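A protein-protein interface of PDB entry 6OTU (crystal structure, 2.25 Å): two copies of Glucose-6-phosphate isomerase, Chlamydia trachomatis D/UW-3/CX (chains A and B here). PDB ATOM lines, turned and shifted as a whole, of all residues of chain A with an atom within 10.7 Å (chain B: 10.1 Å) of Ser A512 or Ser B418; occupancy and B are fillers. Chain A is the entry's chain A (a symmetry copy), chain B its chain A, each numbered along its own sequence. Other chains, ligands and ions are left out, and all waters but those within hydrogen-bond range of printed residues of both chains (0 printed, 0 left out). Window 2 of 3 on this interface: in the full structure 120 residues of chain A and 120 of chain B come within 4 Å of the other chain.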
ATOM      1  N   ILE A 187       9.538 -18.007  -9.066  1.00  0.00           N
ATOM      2  CA  ILE A 187       9.596 -19.448  -9.243  1.00  0.00           C
ATOM      3  C   ILE A 187       8.196 -20.049  -9.356  1.00  0.00           C
ATOM      4  O   ILE A 187       8.051 -21.159  -9.881  1.00  0.00           O
ATOM      5  CB  ILE A 187      10.393 -20.144  -8.126  1.00  0.00           C
ATOM      6  CG1 ILE A 187      10.876 -21.499  -8.655  1.00  0.00           C
ATOM      7  CG2 ILE A 187       9.580 -20.233  -6.828  1.00  0.00           C
ATOM      8  CD1 ILE A 187      11.391 -22.399  -7.634  1.00  0.00           C
ATOM      9  N   LEU A 216      18.043 -19.806  -8.015  1.00  0.00           N
ATOM     10  CA  LEU A 216      17.077 -20.864  -8.319  1.00  0.00           C
ATOM     11  C   LEU A 216      16.049 -20.441  -9.371  1.00  0.00           C
ATOM     12  O   LEU A 216      15.738 -21.212 -10.289  1.00  0.00           O
ATOM     13  CB  LEU A 216      16.363 -21.297  -7.042  1.00  0.00           C
ATOM     14  CG  LEU A 216      15.122 -22.166  -7.255  1.00  0.00           C
ATOM     15  CD1 LEU A 216      15.519 -23.477  -7.905  1.00  0.00           C
ATOM     16  CD2 LEU A 216      14.368 -22.401  -5.940  1.00  0.00           C
ATOM     17  N   ALA A 219      17.090 -20.169 -13.062  1.00  0.00           N
ATOM     18  CA  ALA A 219      17.498 -21.498 -13.520  1.00  0.00           C
ATOM     19  C   ALA A 219      16.292 -22.401 -13.733  1.00  0.00           C
ATOM     20  O   ALA A 219      16.219 -23.123 -14.735  1.00  0.00           O
ATOM     21  CB  ALA A 219      18.456 -22.139 -12.528  1.00  0.00           C
ATOM     22  N   ALA A 220      15.336 -22.378 -12.804  1.00  0.00           N
ATOM     23  CA  ALA A 220      14.129 -23.163 -13.023  1.00  0.00           C
ATOM     24  C   ALA A 220      13.345 -22.619 -14.207  1.00  0.00           C
ATOM     25  O   ALA A 220      12.813 -23.388 -15.014  1.00  0.00           O
ATOM     26  CB  ALA A 220      13.271 -23.189 -11.759  1.00  0.00           C
ATOM     27  N   GLU A 223      15.002 -23.465 -17.610  1.00  0.00           N
ATOM     28  CA  GLU A 223      14.758 -24.865 -17.943  1.00  0.00           C
ATOM     29  C   GLU A 223      13.327 -25.069 -18.433  1.00  0.00           C
ATOM     30  O   GLU A 223      13.104 -25.794 -19.407  1.00  0.00           O
ATOM     31  CB  GLU A 223      15.073 -25.759 -16.742  1.00  0.00           C
ATOM     32  CG  GLU A 223      14.863 -27.250 -16.987  1.00  0.00           C
ATOM     33  CD  GLU A 223      15.714 -27.804 -18.125  1.00  0.00           C
ATOM     34  OE1 GLU A 223      16.784 -27.219 -18.412  1.00  0.00           O
ATOM     35  OE2 GLU A 223      15.306 -28.830 -18.726  1.00  0.00           O
ATOM     36  N   GLN A 227      12.524 -26.471 -22.316  1.00  0.00           N
ATOM     37  CA  GLN A 227      11.658 -27.611 -22.601  1.00  0.00           C
ATOM     38  C   GLN A 227      10.551 -27.236 -23.571  1.00  0.00           C
ATOM     39  O   GLN A 227      10.187 -28.037 -24.439  1.00  0.00           O
ATOM     40  CB  GLN A 227      11.066 -28.170 -21.309  1.00  0.00           C
ATOM     41  CG  GLN A 227      12.108 -28.460 -20.250  1.00  0.00           C
ATOM     42  CD  GLN A 227      11.940 -29.802 -19.588  1.00  0.00           C
ATOM     43  OE1 GLN A 227      11.613 -29.887 -18.402  1.00  0.00           O
ATOM     44  NE2 GLN A 227      12.175 -30.866 -20.348  1.00  0.00           N
ATOM     45  N   ALA A 504      16.426 -21.312   0.306  1.00  0.00           N
ATOM     46  CA  ALA A 504      15.913 -21.970  -0.894  1.00  0.00           C
ATOM     47  C   ALA A 504      16.702 -23.233  -1.214  1.00  0.00           C
ATOM     48  O   ALA A 504      16.111 -24.259  -1.571  1.00  0.00           O
ATOM     49  CB  ALA A 504      15.940 -21.013  -2.087  1.00  0.00           C
ATOM     50  N   THR A 505      18.035 -23.171  -1.108  1.00  0.00           N
ATOM     51  CA  THR A 505      18.859 -24.364  -1.293  1.00  0.00           C
ATOM     52  C   THR A 505      18.485 -25.453  -0.297  1.00  0.00           C
ATOM     53  O   THR A 505      18.416 -26.632  -0.653  1.00  0.00           O
ATOM     54  CB  THR A 505      20.336 -24.008  -1.146  1.00  0.00           C
ATOM     55  OG1 THR A 505      20.715 -23.140  -2.214  1.00  0.00           O
ATOM     56  CG2 THR A 505      21.209 -25.264  -1.158  1.00  0.00           C
ATOM     57  N   GLN A 506      18.213 -25.074   0.954  1.00  0.00           N
ATOM     58  CA  GLN A 506      17.991 -26.072   1.995  1.00  0.00           C
ATOM     59  C   GLN A 506      16.599 -26.690   1.896  1.00  0.00           C
ATOM     60  O   GLN A 506      16.443 -27.898   2.114  1.00  0.00           O
ATOM     61  CB  GLN A 506      18.235 -25.449   3.369  1.00  0.00           C
ATOM     62  CG  GLN A 506      19.654 -24.893   3.501  1.00  0.00           C
ATOM     63  CD  GLN A 506      19.930 -24.231   4.835  1.00  0.00           C
ATOM     64  OE1 GLN A 506      19.009 -23.822   5.545  1.00  0.00           O
ATOM     65  NE2 GLN A 506      21.210 -24.106   5.177  1.00  0.00           N
ATOM     66  N   ILE A 507      15.576 -25.892   1.561  1.00  0.00           N
ATOM     67  CA  ILE A 507      14.245 -26.482   1.432  1.00  0.00           C
ATOM     68  C   ILE A 507      14.186 -27.412   0.223  1.00  0.00           C
ATOM     69  O   ILE A 507      13.409 -28.378   0.212  1.00  0.00           O
ATOM     70  CB  ILE A 507      13.160 -25.390   1.372  1.00  0.00           C
ATOM     71  CG1 ILE A 507      13.393 -24.433   0.198  1.00  0.00           C
ATOM     72  CG2 ILE A 507      13.104 -24.643   2.683  1.00  0.00           C
ATOM     73  CD1 ILE A 507      12.647 -24.820  -1.081  1.00  0.00           C
ATOM     74  N   ILE A 508      14.993 -27.136  -0.808  1.00  0.00           N
ATOM     75  CA  ILE A 508      15.150 -28.071  -1.921  1.00  0.00           C
ATOM     76  C   ILE A 508      15.716 -29.397  -1.422  1.00  0.00           C
ATOM     77  O   ILE A 508      15.164 -30.473  -1.696  1.00  0.00           O
ATOM     78  CB  ILE A 508      16.042 -27.455  -3.018  1.00  0.00           C
ATOM     79  CG1 ILE A 508      15.234 -26.486  -3.886  1.00  0.00           C
ATOM     80  CG2 ILE A 508      16.691 -28.549  -3.849  1.00  0.00           C
ATOM     81  CD1 ILE A 508      16.076 -25.554  -4.686  1.00  0.00           C
ATOM     82  N   GLY A 509      16.823 -29.339  -0.675  1.00  0.00           N
ATOM     83  CA  GLY A 509      17.388 -30.558  -0.114  1.00  0.00           C
ATOM     84  C   GLY A 509      16.435 -31.278   0.824  1.00  0.00           C
ATOM     85  O   GLY A 509      16.411 -32.511   0.870  1.00  0.00           O
ATOM     86  N   ILE A 510      15.631 -30.519   1.582  1.00  0.00           N
ATOM     87  CA  ILE A 510      14.691 -31.125   2.524  1.00  0.00           C
ATOM     88  C   ILE A 510      13.598 -31.891   1.786  1.00  0.00           C
ATOM     89  O   ILE A 510      13.045 -32.860   2.316  1.00  0.00           O
ATOM     90  CB  ILE A 510      14.092 -30.054   3.456  1.00  0.00           C
ATOM     91  N   MET A 511      13.273 -31.480   0.559  1.00  0.00           N
ATOM     92  CA  MET A 511      12.233 -32.111  -0.243  1.00  0.00           C
ATOM     93  C   MET A 511      12.786 -33.099  -1.271  1.00  0.00           C
ATOM     94  O   MET A 511      12.004 -33.692  -2.027  1.00  0.00           O
ATOM     95  CB  MET A 511      11.380 -31.035  -0.937  1.00  0.00           C
ATOM     96  CG  MET A 511      10.313 -30.427  -0.027  1.00  0.00           C
ATOM     97  SD  MET A 511       9.473 -28.925  -0.604  1.00  0.00           S
ATOM     98  CE  MET A 511       9.595 -29.028  -2.390  1.00  0.00           C
ATOM     99  N   SER A 512      14.103 -33.307  -1.299  1.00  0.00           N
ATOM    100  CA  SER A 512      14.731 -34.242  -2.227  1.00  0.00           C
ATOM    101  C   SER A 512      15.130 -35.542  -1.523  1.00  0.00           C
ATOM    102  O   SER A 512      14.310 -36.177  -0.862  1.00  0.00           O
ATOM    103  CB  SER A 512      15.962 -33.603  -2.874  1.00  0.00           C
ATOM    104  OG  SER A 512      17.099 -33.716  -2.029  1.00  0.00           O
ATOM    105  N   PHE A 519      19.435 -28.043   9.243  1.00  0.00           N
ATOM    106  CA  PHE A 519      19.416 -26.589   9.376  1.00  0.00           C
ATOM    107  C   PHE A 519      18.309 -26.139  10.334  1.00  0.00           C
ATOM    108  O   PHE A 519      17.370 -26.893  10.613  1.00  0.00           O
ATOM    109  CB  PHE A 519      19.280 -25.925   7.992  1.00  0.00           C
ATOM    110  CG  PHE A 519      18.012 -26.253   7.246  1.00  0.00           C
ATOM    111  CD1 PHE A 519      17.881 -27.453   6.569  1.00  0.00           C
ATOM    112  CD2 PHE A 519      16.968 -25.328   7.174  1.00  0.00           C
ATOM    113  CE1 PHE A 519      16.722 -27.751   5.870  1.00  0.00           C
ATOM    114  CE2 PHE A 519      15.803 -25.620   6.472  1.00  0.00           C
ATOM    115  CZ  PHE A 519      15.680 -26.834   5.822  1.00  0.00           C
ATOM    116  N   VAL A 525       9.902 -26.427   9.865  1.00  0.00           N
ATOM    117  CA  VAL A 525       9.284 -26.531   8.539  1.00  0.00           C
ATOM    118  C   VAL A 525       8.448 -27.803   8.431  1.00  0.00           C
ATOM    119  O   VAL A 525       7.327 -27.780   7.904  1.00  0.00           O
ATOM    120  CB  VAL A 525      10.355 -26.463   7.428  1.00  0.00           C
ATOM    121  CG1 VAL A 525       9.806 -26.982   6.105  1.00  0.00           C
ATOM    122  CG2 VAL A 525      10.860 -25.036   7.227  1.00  0.00           C
ATOM    123  N   LEU A 526       8.963 -28.925   8.941  1.00  0.00           N
ATOM    124  CA  LEU A 526       8.227 -30.187   8.848  1.00  0.00           C
ATOM    125  C   LEU A 526       6.873 -30.107   9.546  1.00  0.00           C
ATOM    126  O   LEU A 526       5.863 -30.588   9.018  1.00  0.00           O
ATOM    127  CB  LEU A 526       9.050 -31.332   9.443  1.00  0.00           C
ATOM    128  CG  LEU A 526      10.391 -31.639   8.779  1.00  0.00           C
ATOM    129  CD1 LEU A 526      10.951 -32.994   9.251  1.00  0.00           C
ATOM    130  CD2 LEU A 526      10.250 -31.585   7.259  1.00  0.00           C
ATOM    131  N   PHE A 529       4.567 -27.804   7.732  1.00  0.00           N
ATOM    132  CA  PHE A 529       4.120 -28.516   6.540  1.00  0.00           C
ATOM    133  C   PHE A 529       2.947 -29.428   6.840  1.00  0.00           C
ATOM    134  O   PHE A 529       2.008 -29.511   6.042  1.00  0.00           O
ATOM    135  CB  PHE A 529       5.265 -29.326   5.931  1.00  0.00           C
ATOM    136  CG  PHE A 529       5.983 -28.612   4.822  1.00  0.00           C
ATOM    137  CD1 PHE A 529       5.815 -27.250   4.644  1.00  0.00           C
ATOM    138  CD2 PHE A 529       6.828 -29.301   3.963  1.00  0.00           C
ATOM    139  CE1 PHE A 529       6.476 -26.579   3.632  1.00  0.00           C
ATOM    140  CE2 PHE A 529       7.496 -28.637   2.943  1.00  0.00           C
ATOM    141  CZ  PHE A 529       7.316 -27.270   2.777  1.00  0.00           C
ATOM    142  N   CYS B 415       7.119 -28.597 -13.362  1.00  0.00           N
ATOM    143  CA  CYS B 415       8.380 -29.212 -13.740  1.00  0.00           C
ATOM    144  C   CYS B 415       8.986 -29.804 -12.482  1.00  0.00           C
ATOM    145  O   CYS B 415       9.045 -29.125 -11.453  1.00  0.00           O
ATOM    146  CB  CYS B 415       9.320 -28.157 -14.344  1.00  0.00           C
ATOM    147  SG  CYS B 415      10.869 -28.752 -14.994  1.00  0.00           S
ATOM    148  N   VAL B 416       9.416 -31.059 -12.553  1.00  0.00           N
ATOM    149  CA  VAL B 416      10.104 -31.696 -11.434  1.00  0.00           C
ATOM    150  C   VAL B 416      11.600 -31.462 -11.583  1.00  0.00           C
ATOM    151  O   VAL B 416      12.194 -31.838 -12.599  1.00  0.00           O
ATOM    152  CB  VAL B 416       9.791 -33.194 -11.362  1.00  0.00           C
ATOM    153  CG1 VAL B 416      10.508 -33.793 -10.179  1.00  0.00           C
ATOM    154  CG2 VAL B 416       8.286 -33.392 -11.244  1.00  0.00           C
ATOM    155  N   LEU B 417      12.206 -30.831 -10.577  1.00  0.00           N
ATOM    156  CA  LEU B 417      13.641 -30.563 -10.564  1.00  0.00           C
ATOM    157  C   LEU B 417      14.175 -30.863  -9.173  1.00  0.00           C
ATOM    158  O   LEU B 417      13.681 -30.300  -8.189  1.00  0.00           O
ATOM    159  CB  LEU B 417      13.949 -29.114 -10.945  1.00  0.00           C
ATOM    160  CG  LEU B 417      13.468 -28.597 -12.300  1.00  0.00           C
ATOM    161  CD1 LEU B 417      13.746 -27.093 -12.398  1.00  0.00           C
ATOM    162  CD2 LEU B 417      14.134 -29.355 -13.433  1.00  0.00           C
ATOM    163  N   SER B 418      15.170 -31.756  -9.102  1.00  0.00           N
ATOM    164  CA  SER B 418      15.772 -32.200  -7.841  1.00  0.00           C
ATOM    165  C   SER B 418      14.741 -32.751  -6.855  1.00  0.00           C
ATOM    166  O   SER B 418      14.846 -32.554  -5.643  1.00  0.00           O
ATOM    167  CB  SER B 418      16.598 -31.086  -7.198  1.00  0.00           C
ATOM    168  OG  SER B 418      17.371 -30.410  -8.177  1.00  0.00           O
ATOM    169  N   GLY B 419      13.754 -33.480  -7.371  1.00  0.00           N
ATOM    170  CA  GLY B 419      12.787 -34.155  -6.530  1.00  0.00           C
ATOM    171  C   GLY B 419      11.552 -33.359  -6.151  1.00  0.00           C
ATOM    172  O   GLY B 419      10.715 -33.878  -5.401  1.00  0.00           O
ATOM    173  N   SER B 420      11.394 -32.123  -6.630  1.00  0.00           N
ATOM    174  CA  SER B 420      10.184 -31.388  -6.282  1.00  0.00           C
ATOM    175  C   SER B 420       9.723 -30.512  -7.442  1.00  0.00           C
ATOM    176  O   SER B 420      10.514 -30.106  -8.303  1.00  0.00           O
ATOM    177  CB  SER B 420      10.381 -30.536  -5.023  1.00  0.00           C
ATOM    178  OG  SER B 420      11.293 -29.476  -5.261  1.00  0.00           O
ATOM    179  N   SER B 421       8.423 -30.238  -7.455  1.00  0.00           N
ATOM    180  CA  SER B 421       7.857 -29.298  -8.400  1.00  0.00           C
ATOM    181  C   SER B 421       8.085 -27.870  -7.915  1.00  0.00           C
ATOM    182  O   SER B 421       8.353 -27.618  -6.735  1.00  0.00           O
ATOM    183  CB  SER B 421       6.367 -29.554  -8.577  1.00  0.00           C
ATOM    184  OG  SER B 421       5.643 -28.956  -7.515  1.00  0.00           O
ATOM    185  N   SER B 422       7.957 -26.927  -8.852  1.00  0.00           N
ATOM    186  CA  SER B 422       8.114 -25.514  -8.525  1.00  0.00           C
ATOM    187  C   SER B 422       6.961 -24.993  -7.666  1.00  0.00           C
ATOM    188  O   SER B 422       7.176 -24.124  -6.816  1.00  0.00           O
ATOM    189  CB  SER B 422       8.244 -24.700  -9.814  1.00  0.00           C
ATOM    190  OG  SER B 422       9.566 -24.785 -10.335  1.00  0.00           O
ATOM    191  N   GLN B 424       5.773 -26.675  -5.281  1.00  0.00           N
ATOM    192  CA  GLN B 424       6.271 -27.043  -3.956  1.00  0.00           C
ATOM    193  C   GLN B 424       7.388 -26.108  -3.502  1.00  0.00           C
ATOM    194  O   GLN B 424       7.377 -25.620  -2.369  1.00  0.00           O
ATOM    195  CB  GLN B 424       6.745 -28.502  -3.951  1.00  0.00           C
ATOM    196  CG  GLN B 424       5.637 -29.487  -4.304  1.00  0.00           C
ATOM    197  CD  GLN B 424       6.141 -30.916  -4.511  1.00  0.00           C
ATOM    198  OE1 GLN B 424       7.173 -31.155  -5.147  1.00  0.00           O
ATOM    199  NE2 GLN B 424       5.405 -31.872  -3.969  1.00  0.00           N
ATOM    200  N   LYS B 425       8.360 -25.837  -4.372  1.00  0.00           N
ATOM    201  CA  LYS B 425       9.408 -24.887  -4.007  1.00  0.00           C
ATOM    202  C   LYS B 425       8.824 -23.529  -3.615  1.00  0.00           C
ATOM    203  O   LYS B 425       9.271 -22.912  -2.643  1.00  0.00           O
ATOM    204  CB  LYS B 425      10.399 -24.740  -5.161  1.00  0.00           C
ATOM    205  CG  LYS B 425      11.167 -26.016  -5.507  1.00  0.00           C
ATOM    206  CD  LYS B 425      12.112 -25.763  -6.674  1.00  0.00           C
ATOM    207  CE  LYS B 425      12.960 -26.978  -6.986  1.00  0.00           C
ATOM    208  NZ  LYS B 425      12.163 -28.023  -7.663  1.00  0.00           N
ATOM    209  N   ALA B 428       7.294 -23.911  -0.064  1.00  0.00           N
ATOM    210  CA  ALA B 428       8.348 -24.163   0.915  1.00  0.00           C
ATOM    211  C   ALA B 428       9.122 -22.894   1.236  1.00  0.00           C
ATOM    212  O   ALA B 428       9.501 -22.664   2.389  1.00  0.00           O
ATOM    213  CB  ALA B 428       9.301 -25.239   0.385  1.00  0.00           C
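SG of Cys B415 is in hydrogen-bond range of OE1 of Gln A227 (3.7 Å).
O of Gly A509 is in hydrogen-bond range of OG of Ser A512 (3.2 Å). The backbone carbonyl oxygen of Leu B417 lies within hydrogen-bond range of the side-chain amino group of Lys B425 (2.8 Å). The side-chain amino group (NZ) of Lys B425 sits at hydrogen-bond distance from the backbone carbonyl oxygen (O) of Ser B420, at 2.7 Å. The backbone NH (N) of Ser B421 lies within hydrogen-bond range of the side-chain amide oxygen (OE1) of Gln B424 (2.8 Å).
O of Ile A187 touches CB of Ser B422, 3.5 Å away. Leu B417 touches Ala A220 (CD1 to CB, 3.98 Å). Ile A507 touches Ala B428. CG1 of Ile A508 touches CE of Lys B425, 3.9 Å away. Gly B419 touches Met A511. CE of Met A511 touches CB of Ser B420, at 3.1 Å. Met A511 touches Lys B425 (CE to N, 3.95 Å). Ala B428 touches Met A511. Ser A512 touches Ser B418 (CB to O, 3.2 Å). Ala B428 touches Phe A529 (CB to CZ, 3.7 Å).
Of chain B, only Ser B418 (3.2 Å) comes within 4 Å of Ser A512. Ser B418 touches one residue of chain A. Gly B419 touches one residue of chain A. Of chain A, only Met A511 (3.1 Å) comes within 4 Å of Ser B420. Of the printed residues of chain B, Gln A227 touches Cys B415 (3.7 Å). Printed residues of chain B within 4 Å of Ile A187: Ser B422 and Lys B425. Of the printed residues of chain A, Leu B417 touches Ala A220 (3.98 Å). Of the printed residues of chain A, Cys B415 touches Gln A227 (3.7 Å). Of the printed residues of chain A, Ala B428 touches Ile A507 (3.7 Å), Met A511 (3.8 Å) and Phe A529 (3.7 Å). Leu A216 touches none of the printed residues of chain B. The nearest residue of chain B that does not touch Ser A512 is Gly B419 (4.7 Å). The nearest residue of chain A that does not touch Ser B418 is Ile A508 (4.2 Å). The nearest printed residue of chain A that does not touch Gln B424 is Phe A529 (5.4 Å).
Of the 19 printed residues of chain A, 8 touch a printed residue of chain B. Hydrophobic or aromatic side chains of chain A within 4 Å of the printed part of chain B: Ile A187, Ala A220, Ile A507, Ile A508, Met A511 and Phe A529. Of the 11 printed residues of chain B, 9 touch a printed residue of chain A. Hydrophobic or aromatic side chains of chain B that line the printed part of chain A: Leu B417 and Ala B428. Among the printed residues, 13 pairs touch across the chains. Among the printed residues, no Asp or Glu carboxylate lies within 4 Å of a Lys or Arg side-chain nitrogen of the other chain.
No position is printed for both chains. Of the 13 pairs that touch across the chains among the printed residues, none has its exchanged pair printed and touching as well.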
